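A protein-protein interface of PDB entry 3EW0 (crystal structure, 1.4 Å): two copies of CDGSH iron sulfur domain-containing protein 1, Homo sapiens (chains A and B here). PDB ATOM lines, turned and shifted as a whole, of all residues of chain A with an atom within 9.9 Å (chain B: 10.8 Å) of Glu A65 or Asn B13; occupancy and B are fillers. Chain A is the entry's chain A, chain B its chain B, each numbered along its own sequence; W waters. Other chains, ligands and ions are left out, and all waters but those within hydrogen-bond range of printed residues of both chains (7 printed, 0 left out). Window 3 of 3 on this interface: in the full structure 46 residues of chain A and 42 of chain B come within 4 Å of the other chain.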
ATOM      1  N   ASN A  13      -1.382  -3.189  24.185  1.00  0.00           N
ATOM      2  CA  ASN A  13      -2.788  -2.799  24.200  1.00  0.00           C
ATOM      3  C   ASN A  13      -3.113  -2.190  25.550  1.00  0.00           C
ATOM      4  O   ASN A  13      -2.312  -2.299  26.486  1.00  0.00           O
ATOM      5  CB  ASN A  13      -3.712  -3.987  23.884  1.00  0.00           C
ATOM      6  CG  ASN A  13      -3.673  -5.075  24.950  1.00  0.00           C
ATOM      7  OD1 ASN A  13      -4.102  -4.861  26.083  1.00  0.00           O
ATOM      8  ND2 ASN A  13      -3.201  -6.260  24.572  1.00  0.00           N
ATOM      9  N   ALA A  15      -6.333  -2.841  26.873  1.00  0.00           N
ATOM     10  CA  ALA A  15      -7.547  -3.550  27.265  1.00  0.00           C
ATOM     11  C   ALA A  15      -7.463  -3.934  28.734  1.00  0.00           C
ATOM     12  O   ALA A  15      -6.369  -4.129  29.264  1.00  0.00           O
ATOM     13  CB  ALA A  15      -7.714  -4.811  26.427  1.00  0.00           C
ATOM     14  N   MET A  16      -8.620  -4.050  29.377  1.00  0.00           N
ATOM     15  CA  MET A  16      -8.673  -4.675  30.695  1.00  0.00           C
ATOM     16  C   MET A  16      -8.279  -6.129  30.558  1.00  0.00           C
ATOM     17  O   MET A  16      -8.554  -6.778  29.553  1.00  0.00           O
ATOM     18  CB  MET A  16     -10.064  -4.561  31.330  1.00  0.00           C
ATOM     19  CG  MET A  16     -10.554  -3.142  31.506  1.00  0.00           C
ATOM     20  SD  MET A  16     -11.926  -3.041  32.678  1.00  0.00           S
ATOM     21  CE  MET A  16     -13.158  -4.147  31.995  1.00  0.00           C
ATOM     22  N   ILE A  17      -7.610  -6.637  31.583  1.00  0.00           N
ATOM     23  CA  ILE A  17      -7.271  -8.053  31.654  1.00  0.00           C
ATOM     24  C   ILE A  17      -8.470  -8.852  32.159  1.00  0.00           C
ATOM     25  O   ILE A  17      -8.826  -9.897  31.617  1.00  0.00           O
ATOM     26  CB  ILE A  17      -6.040  -8.270  32.578  1.00  0.00           C
ATOM     27  CG1 ILE A  17      -4.778  -7.729  31.895  1.00  0.00           C
ATOM     28  CG2 ILE A  17      -5.875  -9.737  32.955  1.00  0.00           C
ATOM     29  CD1 ILE A  17      -3.554  -7.637  32.825  1.00  0.00           C
ATOM     30  N   LEU A  19     -12.268  -9.012  32.291  1.00  0.00           N
ATOM     31  CA  LEU A  19     -13.414  -8.423  31.614  1.00  0.00           C
ATOM     32  C   LEU A  19     -14.653  -8.422  32.493  1.00  0.00           C
ATOM     33  O   LEU A  19     -15.432  -7.463  32.449  1.00  0.00           O
ATOM     34  CB  LEU A  19     -13.701  -9.147  30.297  1.00  0.00           C
ATOM     35  CG  LEU A  19     -12.520  -9.148  29.323  1.00  0.00           C
ATOM     36  CD1 LEU A  19     -12.779 -10.093  28.147  1.00  0.00           C
ATOM     37  CD2 LEU A  19     -12.246  -7.729  28.835  1.00  0.00           C
ATOM     38  N   CYS A  46      -5.334 -15.672  34.379  1.00  0.00           N
ATOM     39  CA  CYS A  46      -5.887 -15.167  33.109  1.00  0.00           C
ATOM     40  C   CYS A  46      -7.238 -14.434  33.293  1.00  0.00           C
ATOM     41  O   CYS A  46      -7.730 -13.819  32.369  1.00  0.00           O
ATOM     42  CB  CYS A  46      -6.055 -16.334  32.106  1.00  0.00           C
ATOM     43  SG  CYS A  46      -7.480 -17.406  32.433  1.00  0.00           S
ATOM     44  N   ARG A  48     -10.245 -15.509  33.387  1.00  0.00           N
ATOM     45  CA  ARG A  48     -11.327 -16.100  32.584  1.00  0.00           C
ATOM     46  C   ARG A  48     -11.986 -17.293  33.249  1.00  0.00           C
ATOM     47  O   ARG A  48     -13.059 -17.714  32.810  1.00  0.00           O
ATOM     48  CB  ARG A  48     -10.869 -16.529  31.176  1.00  0.00           C
ATOM     49  CG  ARG A  48     -10.166 -15.467  30.328  1.00  0.00           C
ATOM     50  CD  ARG A  48     -11.101 -14.470  29.723  1.00  0.00           C
ATOM     51  NE  ARG A  48     -10.367 -13.435  28.988  1.00  0.00           N
ATOM     52  CZ  ARG A  48      -9.854 -12.328  29.530  1.00  0.00           C
ATOM     53  NH1 ARG A  48      -9.990 -12.081  30.827  1.00  0.00           N
ATOM     54  NH2 ARG A  48      -9.189 -11.461  28.774  1.00  0.00           N
ATOM     55  N   ALA A  58      -9.721 -22.357  31.415  1.00  0.00           N
ATOM     56  CA  ALA A  58     -10.157 -21.284  30.523  1.00  0.00           C
ATOM     57  C   ALA A  58      -8.988 -20.604  29.798  1.00  0.00           C
ATOM     58  O   ALA A  58      -9.167 -20.094  28.690  1.00  0.00           O
ATOM     59  CB  ALA A  58     -10.960 -20.231  31.295  1.00  0.00           C
ATOM     60  N   HIS A  59      -7.808 -20.567  30.415  1.00  0.00           N
ATOM     61  CA  HIS A  59      -6.642 -19.957  29.784  1.00  0.00           C
ATOM     62  C   HIS A  59      -6.369 -20.507  28.375  1.00  0.00           C
ATOM     63  O   HIS A  59      -5.942 -19.761  27.491  1.00  0.00           O
ATOM     64  CB  HIS A  59      -5.409 -20.109  30.677  1.00  0.00           C
ATOM     65  CG  HIS A  59      -5.078 -21.523  31.017  1.00  0.00           C
ATOM     66  ND1 HIS A  59      -5.438 -22.121  32.215  1.00  0.00           N
ATOM     67  CD2 HIS A  59      -4.389 -22.449  30.310  1.00  0.00           C
ATOM     68  CE1 HIS A  59      -5.000 -23.370  32.204  1.00  0.00           C
ATOM     69  NE2 HIS A  59      -4.363 -23.593  31.065  1.00  0.00           N
ATOM     70  N   THR A  60      -6.628 -21.796  28.156  1.00  0.00           N
ATOM     71  CA  THR A  60      -6.313 -22.399  26.859  1.00  0.00           C
ATOM     72  C   THR A  60      -7.115 -21.749  25.737  1.00  0.00           C
ATOM     73  O   THR A  60      -6.592 -21.559  24.647  1.00  0.00           O
ATOM     74  CB  THR A  60      -6.541 -23.933  26.827  1.00  0.00           C
ATOM     75  OG1 THR A  60      -7.929 -24.230  26.972  1.00  0.00           O
ATOM     76  CG2 THR A  60      -5.770 -24.624  27.931  1.00  0.00           C
ATOM     77  N   LYS A  61      -8.378 -21.420  26.010  1.00  0.00           N
ATOM     78  CA  LYS A  61      -9.240 -20.774  25.004  1.00  0.00           C
ATOM     79  C   LYS A  61      -8.721 -19.382  24.657  1.00  0.00           C
ATOM     80  O   LYS A  61      -8.663 -19.008  23.493  1.00  0.00           O
ATOM     81  CB  LYS A  61     -10.692 -20.685  25.516  1.00  0.00           C
ATOM     82  CG  LYS A  61     -11.662 -19.962  24.580  1.00  0.00           C
ATOM     83  CD  LYS A  61     -13.104 -20.068  25.104  1.00  0.00           C
ATOM     84  N   HIS A  62      -8.352 -18.629  25.686  1.00  0.00           N
ATOM     85  CA  HIS A  62      -7.747 -17.321  25.518  1.00  0.00           C
ATOM     86  C   HIS A  62      -6.438 -17.380  24.727  1.00  0.00           C
ATOM     87  O   HIS A  62      -6.220 -16.616  23.794  1.00  0.00           O
ATOM     88  CB  HIS A  62      -7.474 -16.697  26.876  1.00  0.00           C
ATOM     89  CG  HIS A  62      -6.537 -15.535  26.808  1.00  0.00           C
ATOM     90  ND1 HIS A  62      -6.932 -14.278  26.408  1.00  0.00           N
ATOM     91  CD2 HIS A  62      -5.206 -15.456  27.034  1.00  0.00           C
ATOM     92  CE1 HIS A  62      -5.887 -13.472  26.409  1.00  0.00           C
ATOM     93  NE2 HIS A  62      -4.824 -14.162  26.783  1.00  0.00           N
ATOM     94  N   ASN A  63      -5.562 -18.293  25.116  1.00  0.00           N
ATOM     95  CA  ASN A  63      -4.277 -18.435  24.420  1.00  0.00           C
ATOM     96  C   ASN A  63      -4.443 -18.773  22.944  1.00  0.00           C
ATOM     97  O   ASN A  63      -3.758 -18.227  22.065  1.00  0.00           O
ATOM     98  CB  ASN A  63      -3.413 -19.510  25.078  1.00  0.00           C
ATOM     99  CG  ASN A  63      -2.829 -19.080  26.409  1.00  0.00           C
ATOM    100  OD1 ASN A  63      -2.767 -17.892  26.736  1.00  0.00           O
ATOM    101  ND2 ASN A  63      -2.412 -20.057  27.204  1.00  0.00           N
ATOM    102  N   GLU A  64      -5.376 -19.665  22.661  1.00  0.00           N
ATOM    103  CA  GLU A  64      -5.623 -20.105  21.312  1.00  0.00           C
ATOM    104  C   GLU A  64      -6.147 -18.933  20.471  1.00  0.00           C
ATOM    105  O   GLU A  64      -5.665 -18.680  19.374  1.00  0.00           O
ATOM    106  CB  GLU A  64      -6.620 -21.255  21.355  1.00  0.00           C
ATOM    107  CG  GLU A  64      -6.961 -21.881  20.042  1.00  0.00           C
ATOM    108  CD  GLU A  64      -7.915 -23.038  20.240  1.00  0.00           C
ATOM    109  OE1 GLU A  64      -9.097 -22.781  20.541  1.00  0.00           O
ATOM    110  OE2 GLU A  64      -7.465 -24.196  20.130  1.00  0.00           O
ATOM    111  N   GLU A  65      -7.109 -18.209  21.025  1.00  0.00           N
ATOM    112  CA  GLU A  65      -7.701 -17.052  20.361  1.00  0.00           C
ATOM    113  C   GLU A  65      -6.715 -15.940  20.040  1.00  0.00           C
ATOM    114  O   GLU A  65      -6.688 -15.442  18.917  1.00  0.00           O
ATOM    115  CB  GLU A  65      -8.773 -16.448  21.254  1.00  0.00           C
ATOM    116  CG  GLU A  65     -10.058 -17.218  21.292  1.00  0.00           C
ATOM    117  CD  GLU A  65     -11.197 -16.366  21.798  1.00  0.00           C
ATOM    118  OE1 GLU A  65     -11.594 -15.429  21.067  1.00  0.00           O
ATOM    119  OE2 GLU A  65     -11.684 -16.631  22.919  1.00  0.00           O
ATOM    120  N   THR A  66      -5.939 -15.531  21.042  1.00  0.00           N
ATOM    121  CA  THR A  66      -5.134 -14.319  20.946  1.00  0.00           C
ATOM    122  C   THR A  66      -3.668 -14.580  20.633  1.00  0.00           C
ATOM    123  O   THR A  66      -2.908 -13.642  20.376  1.00  0.00           O
ATOM    124  CB  THR A  66      -5.190 -13.525  22.246  1.00  0.00           C
ATOM    125  OG1 THR A  66      -4.570 -14.294  23.279  1.00  0.00           O
ATOM    126  CG2 THR A  66      -6.614 -13.229  22.666  1.00  0.00           C
ATOM    127  N   GLY A  67      -3.256 -15.843  20.645  1.00  0.00           N
ATOM    128  CA  GLY A  67      -1.840 -16.181  20.499  1.00  0.00           C
ATOM    129  C   GLY A  67      -1.013 -15.979  21.763  1.00  0.00           C
ATOM    130  O   GLY A  67       0.204 -15.994  21.694  1.00  0.00           O
ATOM    131  N   ASP A  68      -1.675 -15.777  22.896  1.00  0.00           N
ATOM    132  CA  ASP A  68      -1.019 -15.559  24.196  1.00  0.00           C
ATOM    133  C   ASP A  68      -0.458 -16.880  24.754  1.00  0.00           C
ATOM    134  O   ASP A  68      -0.671 -17.958  24.166  1.00  0.00           O
ATOM    135  CB  ASP A  68      -2.038 -14.919  25.170  1.00  0.00           C
ATOM    136  CG  ASP A  68      -1.395 -14.042  26.243  1.00  0.00           C
ATOM    137  OD1 ASP A  68      -0.142 -14.017  26.378  1.00  0.00           O
ATOM    138  OD2 ASP A  68      -2.168 -13.373  26.965  1.00  0.00           O
ATOM    139  N   ASN A  69       0.252 -16.790  25.889  1.00  0.00           N
ATOM    140  CA  ASN A  69       0.923 -17.917  26.493  1.00  0.00           C
ATOM    141  C   ASN A  69       0.800 -17.895  27.993  1.00  0.00           C
ATOM    142  O   ASN A  69       1.750 -18.259  28.693  1.00  0.00           O
ATOM    143  CB  ASN A  69       2.423 -17.926  26.126  1.00  0.00           C
ATOM    144  CG  ASN A  69       3.177 -16.714  26.685  1.00  0.00           C
ATOM    145  OD1 ASN A  69       2.582 -15.671  26.991  1.00  0.00           O
ATOM    146  ND2 ASN A  69       4.496 -16.825  26.737  1.00  0.00           N
ATOM    147  N   VAL A  70      -0.362 -17.477  28.495  1.00  0.00           N
ATOM    148  CA  VAL A  70      -0.561 -17.379  29.928  1.00  0.00           C
ATOM    149  C   VAL A  70      -0.975 -18.731  30.503  1.00  0.00           C
ATOM    150  O   VAL A  70      -1.557 -19.582  29.839  1.00  0.00           O
ATOM    151  CB  VAL A  70      -1.589 -16.247  30.320  1.00  0.00           C
ATOM    152  CG1 VAL A  70      -1.033 -14.863  29.982  1.00  0.00           C
ATOM    153  CG2 VAL A  70      -2.953 -16.474  29.695  1.00  0.00           C
ATOM    154  N   LYS B   9     -19.051  -2.129  16.080  1.00  0.00           N
ATOM    155  CA  LYS B   9     -17.723  -2.527  15.625  1.00  0.00           C
ATOM    156  C   LYS B   9     -17.718  -4.025  15.368  1.00  0.00           C
ATOM    157  O   LYS B   9     -18.614  -4.746  15.814  1.00  0.00           O
ATOM    158  CB  LYS B   9     -16.673  -2.191  16.682  1.00  0.00           C
ATOM    159  N   ASP B  10     -16.691  -4.490  14.666  1.00  0.00           N
ATOM    160  CA  ASP B  10     -16.597  -5.888  14.287  1.00  0.00           C
ATOM    161  C   ASP B  10     -15.140  -6.278  14.030  1.00  0.00           C
ATOM    162  O   ASP B  10     -14.547  -5.870  13.033  1.00  0.00           O
ATOM    163  CB  ASP B  10     -17.456  -6.119  13.043  1.00  0.00           C
ATOM    164  CG  ASP B  10     -17.558  -7.573  12.655  1.00  0.00           C
ATOM    165  OD1 ASP B  10     -17.344  -8.466  13.506  1.00  0.00           O
ATOM    166  OD2 ASP B  10     -17.861  -7.815  11.475  1.00  0.00           O
ATOM    167  N   HIS B  11     -14.571  -7.076  14.931  1.00  0.00           N
ATOM    168  CA  HIS B  11     -13.184  -7.513  14.797  1.00  0.00           C
ATOM    169  C   HIS B  11     -12.895  -8.717  15.685  1.00  0.00           C
ATOM    170  O   HIS B  11     -13.601  -8.953  16.665  1.00  0.00           O
ATOM    171  CB  HIS B  11     -12.228  -6.372  15.152  1.00  0.00           C
ATOM    172  CG  HIS B  11     -12.408  -5.851  16.543  1.00  0.00           C
ATOM    173  ND1 HIS B  11     -11.803  -6.431  17.639  1.00  0.00           N
ATOM    174  CD2 HIS B  11     -13.123  -4.803  17.017  1.00  0.00           C
ATOM    175  CE1 HIS B  11     -12.139  -5.762  18.728  1.00  0.00           C
ATOM    176  NE2 HIS B  11     -12.940  -4.771  18.378  1.00  0.00           N
ATOM    177  N   ARG B  12     -11.857  -9.471  15.327  1.00  0.00           N
ATOM    178  CA  ARG B  12     -11.418 -10.624  16.117  1.00  0.00           C
ATOM    179  C   ARG B  12     -10.780 -10.166  17.427  1.00  0.00           C
ATOM    180  O   ARG B  12     -10.328  -9.022  17.545  1.00  0.00           O
ATOM    181  CB  ARG B  12     -10.424 -11.476  15.319  1.00  0.00           C
ATOM    182  N   ASN B  13     -10.761 -11.061  18.411  1.00  0.00           N
ATOM    183  CA  ASN B  13     -10.103 -10.790  19.688  1.00  0.00           C
ATOM    184  C   ASN B  13      -8.591 -10.982  19.569  1.00  0.00           C
ATOM    185  O   ASN B  13      -8.110 -12.108  19.411  1.00  0.00           O
ATOM    186  CB  ASN B  13     -10.661 -11.696  20.791  1.00  0.00           C
ATOM    187  CG  ASN B  13     -10.004 -11.449  22.144  1.00  0.00           C
ATOM    188  OD1 ASN B  13      -9.649 -10.314  22.484  1.00  0.00           O
ATOM    189  ND2 ASN B  13      -9.844 -12.513  22.927  1.00  0.00           N
ATOM    190  N   LYS B  14      -7.850  -9.879  19.644  1.00  0.00           N
ATOM    191  CA  LYS B  14      -6.390  -9.905  19.493  1.00  0.00           C
ATOM    192  C   LYS B  14      -5.624  -9.487  20.758  1.00  0.00           C
ATOM    193  O   LYS B  14      -4.398  -9.587  20.782  1.00  0.00           O
ATOM    194  CB  LYS B  14      -5.988  -9.001  18.319  1.00  0.00           C
ATOM    195  N   ALA B  15      -6.341  -9.039  21.795  1.00  0.00           N
ATOM    196  CA  ALA B  15      -5.716  -8.500  23.001  1.00  0.00           C
ATOM    197  C   ALA B  15      -5.109  -9.586  23.876  1.00  0.00           C
ATOM    198  O   ALA B  15      -5.825 -10.329  24.567  1.00  0.00           O
ATOM    199  CB  ALA B  15      -6.722  -7.679  23.821  1.00  0.00           C
ATOM    200  N   MET B  16      -3.783  -9.655  23.881  1.00  0.00           N
ATOM    201  CA  MET B  16      -3.076 -10.518  24.818  1.00  0.00           C
ATOM    202  C   MET B  16      -3.095  -9.939  26.246  1.00  0.00           C
ATOM    203  O   MET B  16      -3.123  -8.720  26.453  1.00  0.00           O
ATOM    204  CB  MET B  16      -1.636 -10.746  24.358  1.00  0.00           C
ATOM    205  CG  MET B  16      -1.545 -11.471  23.023  1.00  0.00           C
ATOM    206  SD  MET B  16       0.093 -12.108  22.729  1.00  0.00           S
ATOM    207  CE  MET B  16       1.057 -10.644  22.922  1.00  0.00           C
ATOM    208  N   ILE B  17      -3.073 -10.834  27.225  1.00  0.00           N
ATOM    209  CA  ILE B  17      -2.955 -10.442  28.625  1.00  0.00           C
ATOM    210  C   ILE B  17      -1.483 -10.180  28.967  1.00  0.00           C
ATOM    211  O   ILE B  17      -1.137  -9.140  29.535  1.00  0.00           O
ATOM    212  CB  ILE B  17      -3.499 -11.542  29.537  1.00  0.00           C
ATOM    213  CG1 ILE B  17      -5.037 -11.562  29.491  1.00  0.00           C
ATOM    214  CG2 ILE B  17      -2.995 -11.314  30.931  1.00  0.00           C
ATOM    215  CD1 ILE B  17      -5.642 -12.861  30.066  1.00  0.00           C
ATOM    216  N   PRO B  26       5.464 -21.473  25.333  1.00  0.00           N
ATOM    217  CA  PRO B  26       4.105 -21.458  24.800  1.00  0.00           C
ATOM    218  C   PRO B  26       2.997 -21.439  25.853  1.00  0.00           C
ATOM    219  O   PRO B  26       1.837 -21.136  25.531  1.00  0.00           O
ATOM    220  CB  PRO B  26       4.048 -22.745  23.981  1.00  0.00           C
ATOM    221  CG  PRO B  26       5.003 -23.638  24.654  1.00  0.00           C
ATOM    222  CD  PRO B  26       6.122 -22.771  25.080  1.00  0.00           C
HETATM  223  O   HOH W   1      -3.864  -6.715  28.068  1.00  0.00           O
HETATM  224  O   HOH W   2      -1.972  -7.874  22.359  1.00  0.00           O
HETATM  225  O   HOH W   3       1.512 -20.250  23.022  1.00  0.00           O
HETATM  226  O   HOH W   4      -0.249 -12.765  19.174  1.00  0.00           O
HETATM  227  O   HOH W   5       2.315 -14.864  23.017  1.00  0.00           O
HETATM  228  O   HOH W   6      -9.531 -13.700  25.914  1.00  0.00           O
HETATM  229  O   HOH W   7      -3.178 -11.266  19.255  1.00  0.00           O
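The side-chain amide nitrogen of Asn A13 lies within hydrogen-bond range of the backbone carbonyl oxygen of Met B16 (3.1 Å). The backbone NH (N) of Ile B17 sits at hydrogen-bond distance from the side-chain carboxylate (OD2) of Asp A68, 2.7 Å away.
Water W7 lies within hydrogen-bond range of O of Lys B14 (2.6 Å) and O of Thr A66 (2.6 Å). Water W1 bridges the backbone carbonyl oxygen of Met B16 (2.7 Å) and the side-chain amide oxygen of Asn A13 (2.7 Å). Water W3 bridges the backbone carbonyl oxygen of Pro B26 and the backbone carbonyl oxygen of Asp A68. Water W6 lies within hydrogen-bond range of ND1 of His A62 (2.7 Å), NE of Arg A48 (3.2 Å) and ND2 of Asn B13 (3.2 Å). Water W5 bridges the backbone carbonyl oxygen of Gly A67 and the side-chain sulfur of Met B16. Water W4 lies within hydrogen-bond range of the backbone carbonyl oxygen (O) of Thr A66 (3.0 Å) and the side-chain sulfur (SD) of Met B16 (3.6 Å).
His A59 touches none of the printed residues of chain B. Lys A61 touches none of the printed residues of chain B. Of the printed residues of chain B, His A62 touches Ala B15 (3.6 Å) and Ile B17 (3.6 Å). Glu A65 touches just one residue of chain B: Asn B13 (3.7 Å). Printed residues of chain B within 4 Å of Asp A68: Met B16 (3.6 Å) and Ile B17 (2.7 Å). No residue of chain A comes within 4 Å of Arg B12. Asn B13 touches just these residues of chain A: Glu A65 and Thr A66. No residue of chain A comes within 4 Å of Lys B14. Printed residues of chain A within 4 Å of Ala B15: Asn A13, His A62 and Thr A66. Of the printed residues of chain A, Pro B26 touches Asn A69 (3.3 Å).
N of Asn A69 lies within hydrogen-bond range of OD1 of Asn A63, at 3.3 Å. The guanidinium group of Arg A48 is in hydrogen-bond range of the backbone carbonyl oxygen of Ile A17, at 2.6 Å. O of His A62 sits at hydrogen-bond distance from OG1 of Thr A66 (2.9 Å). The side-chain amide oxygen (OD1) of Asn A13 lies within hydrogen-bond range of the backbone NH (N) of Ala A15 (3.1 Å). The side-chain amide oxygen (OD1) of Asn A63 lies close to the backbone carbonyl oxygen (O) of Asp A68 (3.3 Å). The backbone NH (N) of Asp A68 lies close to the side-chain hydroxyl (OG1) of Thr A66.
Among the printed residues, merely in contact across the chains: Asn A13 with Ala B15, Ile A17 with Ile B17, Cys A46 with Ile B17, His A62 with Ala B15, His A62 with Ile B17, Glu A65 with Asn B13, Thr A66 with Asn B13, Thr A66 with Ala B15, Thr A66 with Met B16, Asp A68 with Met B16 and Asn A69 with Pro B26.
Asn A13 touches Ala B15, but with the chains exchanged Ala A15 does not touch Asn B13 (7.0 Å). Asn A13 touches Met B16, but with the chains exchanged Met A16 does not touch Asn B13 (8.0 Å). Ile B17 touches its own counterpart, Ile A17. Positions printed for both chains: 13, 15, 16 and 17. Of the 13 pairs that touch across the chains among the printed residues, 1 has its exchanged pair printed and touching as well.
Printed residues of chain A that touch a printed residue of chain B: Asn A13, Ile A17, Cys A46, His A62, Glu A65, Thr A66, Asp A68 and Asn A69.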
